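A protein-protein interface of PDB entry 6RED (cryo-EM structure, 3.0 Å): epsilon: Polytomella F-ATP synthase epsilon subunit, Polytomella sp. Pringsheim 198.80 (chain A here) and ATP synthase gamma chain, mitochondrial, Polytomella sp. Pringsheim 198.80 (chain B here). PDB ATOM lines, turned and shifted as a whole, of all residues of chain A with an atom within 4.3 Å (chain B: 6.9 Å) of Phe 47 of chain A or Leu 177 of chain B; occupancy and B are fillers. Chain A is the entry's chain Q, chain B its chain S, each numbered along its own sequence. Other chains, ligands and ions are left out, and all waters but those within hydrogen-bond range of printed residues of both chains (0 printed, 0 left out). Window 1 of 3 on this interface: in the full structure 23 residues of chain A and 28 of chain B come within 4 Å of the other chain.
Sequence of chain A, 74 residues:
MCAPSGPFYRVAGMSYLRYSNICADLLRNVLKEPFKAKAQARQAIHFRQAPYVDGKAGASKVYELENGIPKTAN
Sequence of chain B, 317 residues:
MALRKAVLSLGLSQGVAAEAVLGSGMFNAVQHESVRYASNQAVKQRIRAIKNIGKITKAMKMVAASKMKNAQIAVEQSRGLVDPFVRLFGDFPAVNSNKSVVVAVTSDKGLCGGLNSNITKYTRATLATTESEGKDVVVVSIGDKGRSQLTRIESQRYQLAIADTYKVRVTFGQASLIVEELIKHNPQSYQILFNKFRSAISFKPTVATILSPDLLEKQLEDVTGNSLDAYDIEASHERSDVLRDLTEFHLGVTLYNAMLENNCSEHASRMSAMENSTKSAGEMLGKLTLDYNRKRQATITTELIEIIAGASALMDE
Printed residues of chain A that touch a printed residue of chain B: Arg 18, Ile 45, His 46, Phe 47, Arg 48 and Tyr 63.
Among the printed residues, 21 pairs touch across the chains.
Among the printed residues, Asp or Glu carboxylates within 4 Å of a Lys or Arg side-chain nitrogen of the other chain: Arg 18 of chain A with Glu 180 of chain B and Arg 48 of chain A with Asp 164 of chain B.
Among the printed residues, merely in contact across the chains: His 46 of chain A with Val 168 of chain B (3.4 Å), Arg 18 of chain A with Leu 177 of chain B (3.4 Å), Phe 47 of chain A with Asp 164 of chain B (3.5 Å), Tyr 63 of chain A with Glu 181 of chain B (3.5 Å), Arg 48 of chain A with Ile 162 of chain B (3.5 Å), His 46 of chain A with Gln 174 of chain B (3.6 Å), Phe 47 of chain A with Ile 162 of chain B (3.7 Å), Phe 47 of chain A with Ala 163 of chain B (3.7 Å), Ile 45 of chain A with Leu 177 of chain B (3.8 Å), Phe 47 of chain A with Ile 178 of chain B (3.9 Å), Phe 47 of chain A with Gln 174 of chain B (3.9 Å), Ile 45 of chain A with Gly 173 of chain B (3.9 Å), Phe 47 of chain A with Glu 181 of chain B (3.9 Å), Tyr 63 of chain A with Leu 177 of chain B (3.9 Å), Ile 45 of chain A with Gln 174 of chain B (3.98 Å), Phe 47 of chain A with Leu 177 of chain B (3.99 Å) and Phe 47 of chain A with Thr 165 of chain B (3.99 Å).
Of the printed residues of chain B, Phe 47 of chain A touches Ile 162, Ala 163, Asp 164, Thr 165, Gln 174, Leu 177, Ile 178 and Glu 181.
Printed residues of chain A within 4 Å of Ile 178 of chain B: Phe 47 (3.9 Å).
Printed residues of chain A within 4 Å of Val 168 of chain B: His 46 (3.4 Å).
Printed residues of chain A within 4 Å of Gln 174 of chain B: Ile 45 (3.98 Å), His 46 (3.6 Å) and Phe 47 (3.9 Å).
Printed residues of chain B within 4 Å of Arg 48 of chain A: Ile 162, Ala 163 and Asp 164.
The nearest printed residue of chain A that does not touch Leu 177 of chain B is Ile 69 of chain A (4.1 Å).
The nearest printed residue of chain A that does not touch Val 168 of chain B is Ile 45 of chain A (6.0 Å).
The side-chain amide nitrogen (NE2) of Gln 174 of chain B is in hydrogen-bond range of the backbone carbonyl oxygen (O) of Thr 165 of chain B, at 3.1 Å.
The backbone carbonyl oxygen (O) of Phe 47 of chain A is in hydrogen-bond range of the backbone NH (N) of Tyr 63 of chain A (2.7 Å).
The side-chain carboxylate (OD1) of Asp 164 of chain B lies within salt-bridge range of the side-chain amino group (NZ) of Lys 167 of chain B (3.4 Å).
NH2 of Arg 18 of chain A lies within salt-bridge range of OE1 of Glu 180 of chain B (2.6 Å).
The guanidinium group of Arg 48 of chain A lies within salt-bridge range of the side-chain carboxylate of Asp 164 of chain B (3.0 Å).
The backbone carbonyl oxygen (O) of Asp 164 of chain B lies close to the backbone carbonyl oxygen (O) of His 46 of chain A.
The backbone NH of Ala 163 of chain B sits at hydrogen-bond distance from the backbone carbonyl oxygen of Arg 48 of chain A.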
ATOM      1  N   ARG A  18      38.375  18.647 -30.801  1.00  0.00           N
ATOM      2  CA  ARG A  18      38.414  17.195 -30.703  1.00  0.00           C
ATOM      3  C   ARG A  18      39.828  16.699 -30.470  1.00  0.00           C
ATOM      4  O   ARG A  18      40.042  15.820 -29.632  1.00  0.00           O
ATOM      5  CB  ARG A  18      37.838  16.565 -31.961  1.00  0.00           C
ATOM      6  CG  ARG A  18      37.703  15.074 -31.850  1.00  0.00           C
ATOM      7  CD  ARG A  18      36.903  14.519 -32.992  1.00  0.00           C
ATOM      8  NE  ARG A  18      35.580  15.117 -33.053  1.00  0.00           N
ATOM      9  CZ  ARG A  18      34.528  14.650 -32.398  1.00  0.00           C
ATOM     10  NH1 ARG A  18      34.645  13.579 -31.630  1.00  0.00           N
ATOM     11  NH2 ARG A  18      33.360  15.257 -32.509  1.00  0.00           N
ATOM     12  N   ILE A  45      30.634  12.735 -20.817  1.00  0.00           N
ATOM     13  CA  ILE A  45      29.807  13.547 -21.697  1.00  0.00           C
ATOM     14  C   ILE A  45      28.401  12.978 -21.660  1.00  0.00           C
ATOM     15  O   ILE A  45      28.159  11.872 -22.157  1.00  0.00           O
ATOM     16  CB  ILE A  45      30.343  13.571 -23.130  1.00  0.00           C
ATOM     17  CG1 ILE A  45      31.736  14.187 -23.164  1.00  0.00           C
ATOM     18  CG2 ILE A  45      29.398  14.334 -24.029  1.00  0.00           C
ATOM     19  CD1 ILE A  45      32.379  14.114 -24.517  1.00  0.00           C
ATOM     20  N   HIS A  46      27.466  13.725 -21.081  1.00  0.00           N
ATOM     21  CA  HIS A  46      26.070  13.308 -21.024  1.00  0.00           C
ATOM     22  C   HIS A  46      25.207  14.487 -21.440  1.00  0.00           C
ATOM     23  O   HIS A  46      24.931  15.359 -20.616  1.00  0.00           O
ATOM     24  CB  HIS A  46      25.686  12.845 -19.647  1.00  0.00           C
ATOM     25  CG  HIS A  46      26.344  11.576 -19.206  1.00  0.00           C
ATOM     26  ND1 HIS A  46      27.434  11.558 -18.365  1.00  0.00           N
ATOM     27  CD2 HIS A  46      26.020  10.282 -19.428  1.00  0.00           C
ATOM     28  CE1 HIS A  46      27.778  10.308 -18.118  1.00  0.00           C
ATOM     29  NE2 HIS A  46      26.934   9.514 -18.751  1.00  0.00           N
ATOM     30  N   PHE A  47      24.769  14.503 -22.694  1.00  0.00           N
ATOM     31  CA  PHE A  47      23.779  15.470 -23.144  1.00  0.00           C
ATOM     32  C   PHE A  47      23.063  14.888 -24.351  1.00  0.00           C
ATOM     33  O   PHE A  47      23.333  13.763 -24.775  1.00  0.00           O
ATOM     34  CB  PHE A  47      24.409  16.836 -23.447  1.00  0.00           C
ATOM     35  CG  PHE A  47      25.154  16.905 -24.740  1.00  0.00           C
ATOM     36  CD1 PHE A  47      26.427  16.388 -24.847  1.00  0.00           C
ATOM     37  CD2 PHE A  47      24.601  17.537 -25.838  1.00  0.00           C
ATOM     38  CE1 PHE A  47      27.114  16.465 -26.032  1.00  0.00           C
ATOM     39  CE2 PHE A  47      25.287  17.613 -27.030  1.00  0.00           C
ATOM     40  CZ  PHE A  47      26.539  17.081 -27.124  1.00  0.00           C
ATOM     41  N   ARG A  48      22.125  15.660 -24.890  1.00  0.00           N
ATOM     42  CA  ARG A  48      21.393  15.285 -26.085  1.00  0.00           C
ATOM     43  C   ARG A  48      21.091  16.539 -26.881  1.00  0.00           C
ATOM     44  O   ARG A  48      21.085  17.648 -26.349  1.00  0.00           O
ATOM     45  CB  ARG A  48      20.099  14.539 -25.744  1.00  0.00           C
ATOM     46  CG  ARG A  48      19.010  15.415 -25.168  1.00  0.00           C
ATOM     47  CD  ARG A  48      17.661  14.725 -25.175  1.00  0.00           C
ATOM     48  NE  ARG A  48      16.573  15.690 -25.313  1.00  0.00           N
ATOM     49  CZ  ARG A  48      15.970  16.288 -24.293  1.00  0.00           C
ATOM     50  NH1 ARG A  48      14.991  17.154 -24.515  1.00  0.00           N
ATOM     51  NH2 ARG A  48      16.341  16.026 -23.052  1.00  0.00           N
ATOM     52  N   LYS A  61      19.870  13.113 -30.611  1.00  0.00           N
ATOM     53  CA  LYS A  61      21.178  12.465 -30.680  1.00  0.00           C
ATOM     54  C   LYS A  61      21.694  12.457 -29.247  1.00  0.00           C
ATOM     55  O   LYS A  61      22.274  13.440 -28.782  1.00  0.00           O
ATOM     56  CB  LYS A  61      22.130  13.179 -31.630  1.00  0.00           C
ATOM     57  CG  LYS A  61      23.548  12.605 -31.664  1.00  0.00           C
ATOM     58  CD  LYS A  61      23.579  11.095 -31.843  1.00  0.00           C
ATOM     59  CE  LYS A  61      24.894  10.527 -31.329  1.00  0.00           C
ATOM     60  NZ  LYS A  61      24.955   9.046 -31.425  1.00  0.00           N
ATOM     61  N   VAL A  62      21.470  11.354 -28.551  1.00  0.00           N
ATOM     62  CA  VAL A  62      21.741  11.268 -27.123  1.00  0.00           C
ATOM     63  C   VAL A  62      23.166  10.782 -26.913  1.00  0.00           C
ATOM     64  O   VAL A  62      23.540   9.702 -27.378  1.00  0.00           O
ATOM     65  CB  VAL A  62      20.729  10.340 -26.436  1.00  0.00           C
ATOM     66  CG1 VAL A  62      21.088  10.137 -24.988  1.00  0.00           C
ATOM     67  CG2 VAL A  62      19.340  10.922 -26.540  1.00  0.00           C
ATOM     68  N   TYR A  63      23.962  11.585 -26.219  1.00  0.00           N
ATOM     69  CA  TYR A  63      25.326  11.229 -25.862  1.00  0.00           C
ATOM     70  C   TYR A  63      25.337  10.806 -24.402  1.00  0.00           C
ATOM     71  O   TYR A  63      24.824  11.527 -23.546  1.00  0.00           O
ATOM     72  CB  TYR A  63      26.287  12.400 -26.063  1.00  0.00           C
ATOM     73  CG  TYR A  63      26.418  12.945 -27.472  1.00  0.00           C
ATOM     74  CD1 TYR A  63      25.475  13.823 -27.995  1.00  0.00           C
ATOM     75  CD2 TYR A  63      27.518  12.626 -28.258  1.00  0.00           C
ATOM     76  CE1 TYR A  63      25.607  14.342 -29.269  1.00  0.00           C
ATOM     77  CE2 TYR A  63      27.657  13.142 -29.538  1.00  0.00           C
ATOM     78  CZ  TYR A  63      26.697  13.997 -30.038  1.00  0.00           C
ATOM     79  OH  TYR A  63      26.827  14.512 -31.306  1.00  0.00           O
ATOM     80  N   ILE A  69      35.836  12.208 -25.085  1.00  0.00           N
ATOM     81  CA  ILE A  69      35.352  12.688 -26.377  1.00  0.00           C
ATOM     82  C   ILE A  69      35.590  11.541 -27.359  1.00  0.00           C
ATOM     83  O   ILE A  69      36.529  10.757 -27.160  1.00  0.00           O
ATOM     84  CB  ILE A  69      36.041  14.021 -26.750  1.00  0.00           C
ATOM     85  CG1 ILE A  69      35.227  14.841 -27.753  1.00  0.00           C
ATOM     86  CG2 ILE A  69      37.450  13.819 -27.265  1.00  0.00           C
ATOM     87  CD1 ILE A  69      35.677  16.258 -27.909  1.00  0.00           C
ATOM     88  N   ILE B 162      19.592  21.946 -27.612  1.00  0.00           N
ATOM     89  CA  ILE B 162      20.507  21.086 -26.883  1.00  0.00           C
ATOM     90  C   ILE B 162      20.060  21.034 -25.436  1.00  0.00           C
ATOM     91  O   ILE B 162      20.085  22.051 -24.737  1.00  0.00           O
ATOM     92  CB  ILE B 162      21.948  21.595 -27.011  1.00  0.00           C
ATOM     93  CG1 ILE B 162      22.353  21.567 -28.480  1.00  0.00           C
ATOM     94  CG2 ILE B 162      22.879  20.736 -26.207  1.00  0.00           C
ATOM     95  CD1 ILE B 162      23.523  22.383 -28.803  1.00  0.00           C
ATOM     96  N   ALA B 163      19.651  19.860 -24.986  1.00  0.00           N
ATOM     97  CA  ALA B 163      19.138  19.697 -23.641  1.00  0.00           C
ATOM     98  C   ALA B 163      19.928  18.609 -22.942  1.00  0.00           C
ATOM     99  O   ALA B 163      20.918  18.104 -23.471  1.00  0.00           O
ATOM    100  CB  ALA B 163      17.645  19.370 -23.649  1.00  0.00           C
ATOM    101  N   ASP B 164      19.484  18.278 -21.727  1.00  0.00           N
ATOM    102  CA  ASP B 164      20.118  17.304 -20.831  1.00  0.00           C
ATOM    103  C   ASP B 164      21.576  17.639 -20.542  1.00  0.00           C
ATOM    104  O   ASP B 164      22.366  16.750 -20.234  1.00  0.00           O
ATOM    105  CB  ASP B 164      20.007  15.869 -21.368  1.00  0.00           C
ATOM    106  CG  ASP B 164      18.677  15.212 -21.031  1.00  0.00           C
ATOM    107  OD1 ASP B 164      17.976  15.701 -20.126  1.00  0.00           O
ATOM    108  OD2 ASP B 164      18.330  14.200 -21.671  1.00  0.00           O
ATOM    109  N   THR B 165      21.953  18.913 -20.620  1.00  0.00           N
ATOM    110  CA  THR B 165      23.351  19.271 -20.434  1.00  0.00           C
ATOM    111  C   THR B 165      23.767  19.240 -18.980  1.00  0.00           C
ATOM    112  O   THR B 165      24.931  18.956 -18.693  1.00  0.00           O
ATOM    113  CB  THR B 165      23.638  20.657 -20.999  1.00  0.00           C
ATOM    114  OG1 THR B 165      22.652  21.574 -20.525  1.00  0.00           O
ATOM    115  CG2 THR B 165      23.613  20.635 -22.506  1.00  0.00           C
ATOM    116  N   TYR B 166      22.848  19.511 -18.060  1.00  0.00           N
ATOM    117  CA  TYR B 166      23.167  19.583 -16.645  1.00  0.00           C
ATOM    118  C   TYR B 166      22.777  18.314 -15.916  1.00  0.00           C
ATOM    119  O   TYR B 166      22.708  18.319 -14.685  1.00  0.00           O
ATOM    120  CB  TYR B 166      22.451  20.768 -16.013  1.00  0.00           C
ATOM    121  CG  TYR B 166      22.613  22.049 -16.765  1.00  0.00           C
ATOM    122  CD1 TYR B 166      23.760  22.804 -16.653  1.00  0.00           C
ATOM    123  CD2 TYR B 166      21.598  22.511 -17.588  1.00  0.00           C
ATOM    124  CE1 TYR B 166      23.896  23.977 -17.349  1.00  0.00           C
ATOM    125  CE2 TYR B 166      21.724  23.683 -18.283  1.00  0.00           C
ATOM    126  CZ  TYR B 166      22.875  24.413 -18.158  1.00  0.00           C
ATOM    127  OH  TYR B 166      23.016  25.588 -18.845  1.00  0.00           O
ATOM    128  N   LYS B 167      22.529  17.232 -16.659  1.00  0.00           N
ATOM    129  CA  LYS B 167      21.889  16.042 -16.105  1.00  0.00           C
ATOM    130  C   LYS B 167      22.775  15.348 -15.086  1.00  0.00           C
ATOM    131  O   LYS B 167      22.277  14.807 -14.094  1.00  0.00           O
ATOM    132  CB  LYS B 167      21.516  15.086 -17.229  1.00  0.00           C
ATOM    133  CG  LYS B 167      20.086  15.209 -17.659  1.00  0.00           C
ATOM    134  CD  LYS B 167      19.154  14.842 -16.519  1.00  0.00           C
ATOM    135  CE  LYS B 167      17.724  15.272 -16.806  1.00  0.00           C
ATOM    136  NZ  LYS B 167      17.584  16.749 -16.934  1.00  0.00           N
ATOM    137  N   VAL B 168      24.088  15.369 -15.299  1.00  0.00           N
ATOM    138  CA  VAL B 168      25.060  14.991 -14.278  1.00  0.00           C
ATOM    139  C   VAL B 168      25.978  16.161 -13.914  1.00  0.00           C
ATOM    140  O   VAL B 168      25.937  16.659 -12.790  1.00  0.00           O
ATOM    141  CB  VAL B 168      25.864  13.746 -14.709  1.00  0.00           C
ATOM    142  CG1 VAL B 168      25.106  12.503 -14.338  1.00  0.00           C
ATOM    143  CG2 VAL B 168      26.035  13.738 -16.182  1.00  0.00           C
ATOM    144  N   PHE B 172      34.202  20.003 -20.115  1.00  0.00           N
ATOM    145  CA  PHE B 172      34.723  20.730 -21.262  1.00  0.00           C
ATOM    146  C   PHE B 172      34.570  19.954 -22.559  1.00  0.00           C
ATOM    147  O   PHE B 172      34.448  20.565 -23.621  1.00  0.00           O
ATOM    148  CB  PHE B 172      36.185  21.092 -21.052  1.00  0.00           C
ATOM    149  CG  PHE B 172      36.678  22.095 -22.026  1.00  0.00           C
ATOM    150  CD1 PHE B 172      37.386  21.709 -23.143  1.00  0.00           C
ATOM    151  CD2 PHE B 172      36.392  23.422 -21.855  1.00  0.00           C
ATOM    152  CE1 PHE B 172      37.809  22.627 -24.047  1.00  0.00           C
ATOM    153  CE2 PHE B 172      36.821  24.341 -22.752  1.00  0.00           C
ATOM    154  CZ  PHE B 172      37.528  23.941 -23.851  1.00  0.00           C
ATOM    155  N   GLY B 173      34.590  18.623 -22.509  1.00  0.00           N
ATOM    156  CA  GLY B 173      34.353  17.855 -23.719  1.00  0.00           C
ATOM    157  C   GLY B 173      32.927  17.970 -24.204  1.00  0.00           C
ATOM    158  O   GLY B 173      32.671  17.925 -25.409  1.00  0.00           O
ATOM    159  N   GLN B 174      31.992  18.160 -23.281  1.00  0.00           N
ATOM    160  CA  GLN B 174      30.600  18.378 -23.641  1.00  0.00           C
ATOM    161  C   GLN B 174      30.426  19.714 -24.346  1.00  0.00           C
ATOM    162  O   GLN B 174      29.784  19.798 -25.402  1.00  0.00           O
ATOM    163  CB  GLN B 174      29.761  18.292 -22.373  1.00  0.00           C
ATOM    164  CG  GLN B 174      28.352  18.785 -22.468  1.00  0.00           C
ATOM    165  CD  GLN B 174      27.674  18.713 -21.133  1.00  0.00           C
ATOM    166  OE1 GLN B 174      27.702  17.681 -20.473  1.00  0.00           O
ATOM    167  NE2 GLN B 174      27.082  19.809 -20.715  1.00  0.00           N
ATOM    168  N   ALA B 175      31.032  20.766 -23.792  1.00  0.00           N
ATOM    169  CA  ALA B 175      31.034  22.069 -24.441  1.00  0.00           C
ATOM    170  C   ALA B 175      31.784  22.035 -25.760  1.00  0.00           C
ATOM    171  O   ALA B 175      31.431  22.761 -26.688  1.00  0.00           O
ATOM    172  CB  ALA B 175      31.658  23.107 -23.522  1.00  0.00           C
ATOM    173  N   SER B 176      32.797  21.179 -25.866  1.00  0.00           N
ATOM    174  CA  SER B 176      33.531  21.022 -27.112  1.00  0.00           C
ATOM    175  C   SER B 176      32.672  20.387 -28.192  1.00  0.00           C
ATOM    176  O   SER B 176      32.723  20.805 -29.351  1.00  0.00           O
ATOM    177  CB  SER B 176      34.770  20.179 -26.861  1.00  0.00           C
ATOM    178  OG  SER B 176      35.573  20.769 -25.861  1.00  0.00           O
ATOM    179  N   LEU B 177      31.879  19.378 -27.831  1.00  0.00           N
ATOM    180  CA  LEU B 177      30.974  18.764 -28.799  1.00  0.00           C
ATOM    181  C   LEU B 177      29.886  19.734 -29.233  1.00  0.00           C
ATOM    182  O   LEU B 177      29.527  19.786 -30.418  1.00  0.00           O
ATOM    183  CB  LEU B 177      30.357  17.499 -28.217  1.00  0.00           C
ATOM    184  CG  LEU B 177      31.266  16.284 -28.195  1.00  0.00           C
ATOM    185  CD1 LEU B 177      30.535  15.090 -27.644  1.00  0.00           C
ATOM    186  CD2 LEU B 177      31.744  15.998 -29.588  1.00  0.00           C
ATOM    187  N   ILE B 178      29.371  20.528 -28.292  1.00  0.00           N
ATOM    188  CA  ILE B 178      28.370  21.533 -28.634  1.00  0.00           C
ATOM    189  C   ILE B 178      28.971  22.605 -29.538  1.00  0.00           C
ATOM    190  O   ILE B 178      28.343  23.048 -30.509  1.00  0.00           O
ATOM    191  CB  ILE B 178      27.773  22.127 -27.347  1.00  0.00           C
ATOM    192  CG1 ILE B 178      26.989  21.056 -26.596  1.00  0.00           C
ATOM    193  CG2 ILE B 178      26.863  23.286 -27.642  1.00  0.00           C
ATOM    194  CD1 ILE B 178      26.615  21.465 -25.206  1.00  0.00           C
ATOM    195  N   VAL B 179      30.220  22.988 -29.277  1.00  0.00           N
ATOM    196  CA  VAL B 179      30.875  23.975 -30.121  1.00  0.00           C
ATOM    197  C   VAL B 179      31.181  23.419 -31.501  1.00  0.00           C
ATOM    198  O   VAL B 179      31.130  24.163 -32.477  1.00  0.00           O
ATOM    199  CB  VAL B 179      32.148  24.475 -29.449  1.00  0.00           C
ATOM    200  N   GLU B 180      31.475  22.120 -31.609  1.00  0.00           N
ATOM    201  CA  GLU B 180      31.659  21.513 -32.924  1.00  0.00           C
ATOM    202  C   GLU B 180      30.358  21.479 -33.709  1.00  0.00           C
ATOM    203  O   GLU B 180      30.361  21.685 -34.928  1.00  0.00           O
ATOM    204  CB  GLU B 180      32.222  20.102 -32.787  1.00  0.00           C
ATOM    205  CG  GLU B 180      33.693  20.057 -32.434  1.00  0.00           C
ATOM    206  CD  GLU B 180      34.217  18.647 -32.320  1.00  0.00           C
ATOM    207  OE1 GLU B 180      33.750  17.776 -33.075  1.00  0.00           O
ATOM    208  OE2 GLU B 180      35.096  18.406 -31.472  1.00  0.00           O
ATOM    209  N   GLU B 181      29.238  21.252 -33.025  1.00  0.00           N
ATOM    210  CA  GLU B 181      27.939  21.399 -33.672  1.00  0.00           C
ATOM    211  C   GLU B 181      27.658  22.834 -34.074  1.00  0.00           C
ATOM    212  O   GLU B 181      26.893  23.061 -35.011  1.00  0.00           O
ATOM    213  CB  GLU B 181      26.836  20.920 -32.743  1.00  0.00           C
ATOM    214  CG  GLU B 181      26.950  19.470 -32.399  1.00  0.00           C
ATOM    215  CD  GLU B 181      25.975  19.070 -31.339  1.00  0.00           C
ATOM    216  OE1 GLU B 181      25.207  19.939 -30.886  1.00  0.00           O
ATOM    217  OE2 GLU B 181      26.015  17.898 -30.921  1.00  0.00           O
ATOM    218  N   LEU B 182      28.235  23.804 -33.374  1.00  0.00           N
ATOM    219  CA  LEU B 182      28.115  25.194 -33.793  1.00  0.00           C
ATOM    220  C   LEU B 182      29.024  25.560 -34.956  1.00  0.00           C
ATOM    221  O   LEU B 182      28.651  26.418 -35.755  1.00  0.00           O
ATOM    222  CB  LEU B 182      28.407  26.145 -32.632  1.00  0.00           C
ATOM    223  CG  LEU B 182      27.495  26.140 -31.414  1.00  0.00           C
ATOM    224  CD1 LEU B 182      27.641  27.462 -30.713  1.00  0.00           C
ATOM    225  CD2 LEU B 182      26.056  25.873 -31.783  1.00  0.00           C
ATOM    226  N   LEU B 255      31.731  28.704 -23.980  1.00  0.00           N
ATOM    227  CA  LEU B 255      30.504  27.928 -23.909  1.00  0.00           C
ATOM    228  C   LEU B 255      30.473  27.073 -22.653  1.00  0.00           C
ATOM    229  O   LEU B 255      29.421  26.923 -22.020  1.00  0.00           O
ATOM    230  CB  LEU B 255      30.407  27.072 -25.155  1.00  0.00           C
ATOM    231  CG  LEU B 255      29.055  26.669 -25.667  1.00  0.00           C
ATOM    232  CD1 LEU B 255      28.294  27.911 -26.011  1.00  0.00           C
ATOM    233  CD2 LEU B 255      29.319  25.884 -26.904  1.00  0.00           C
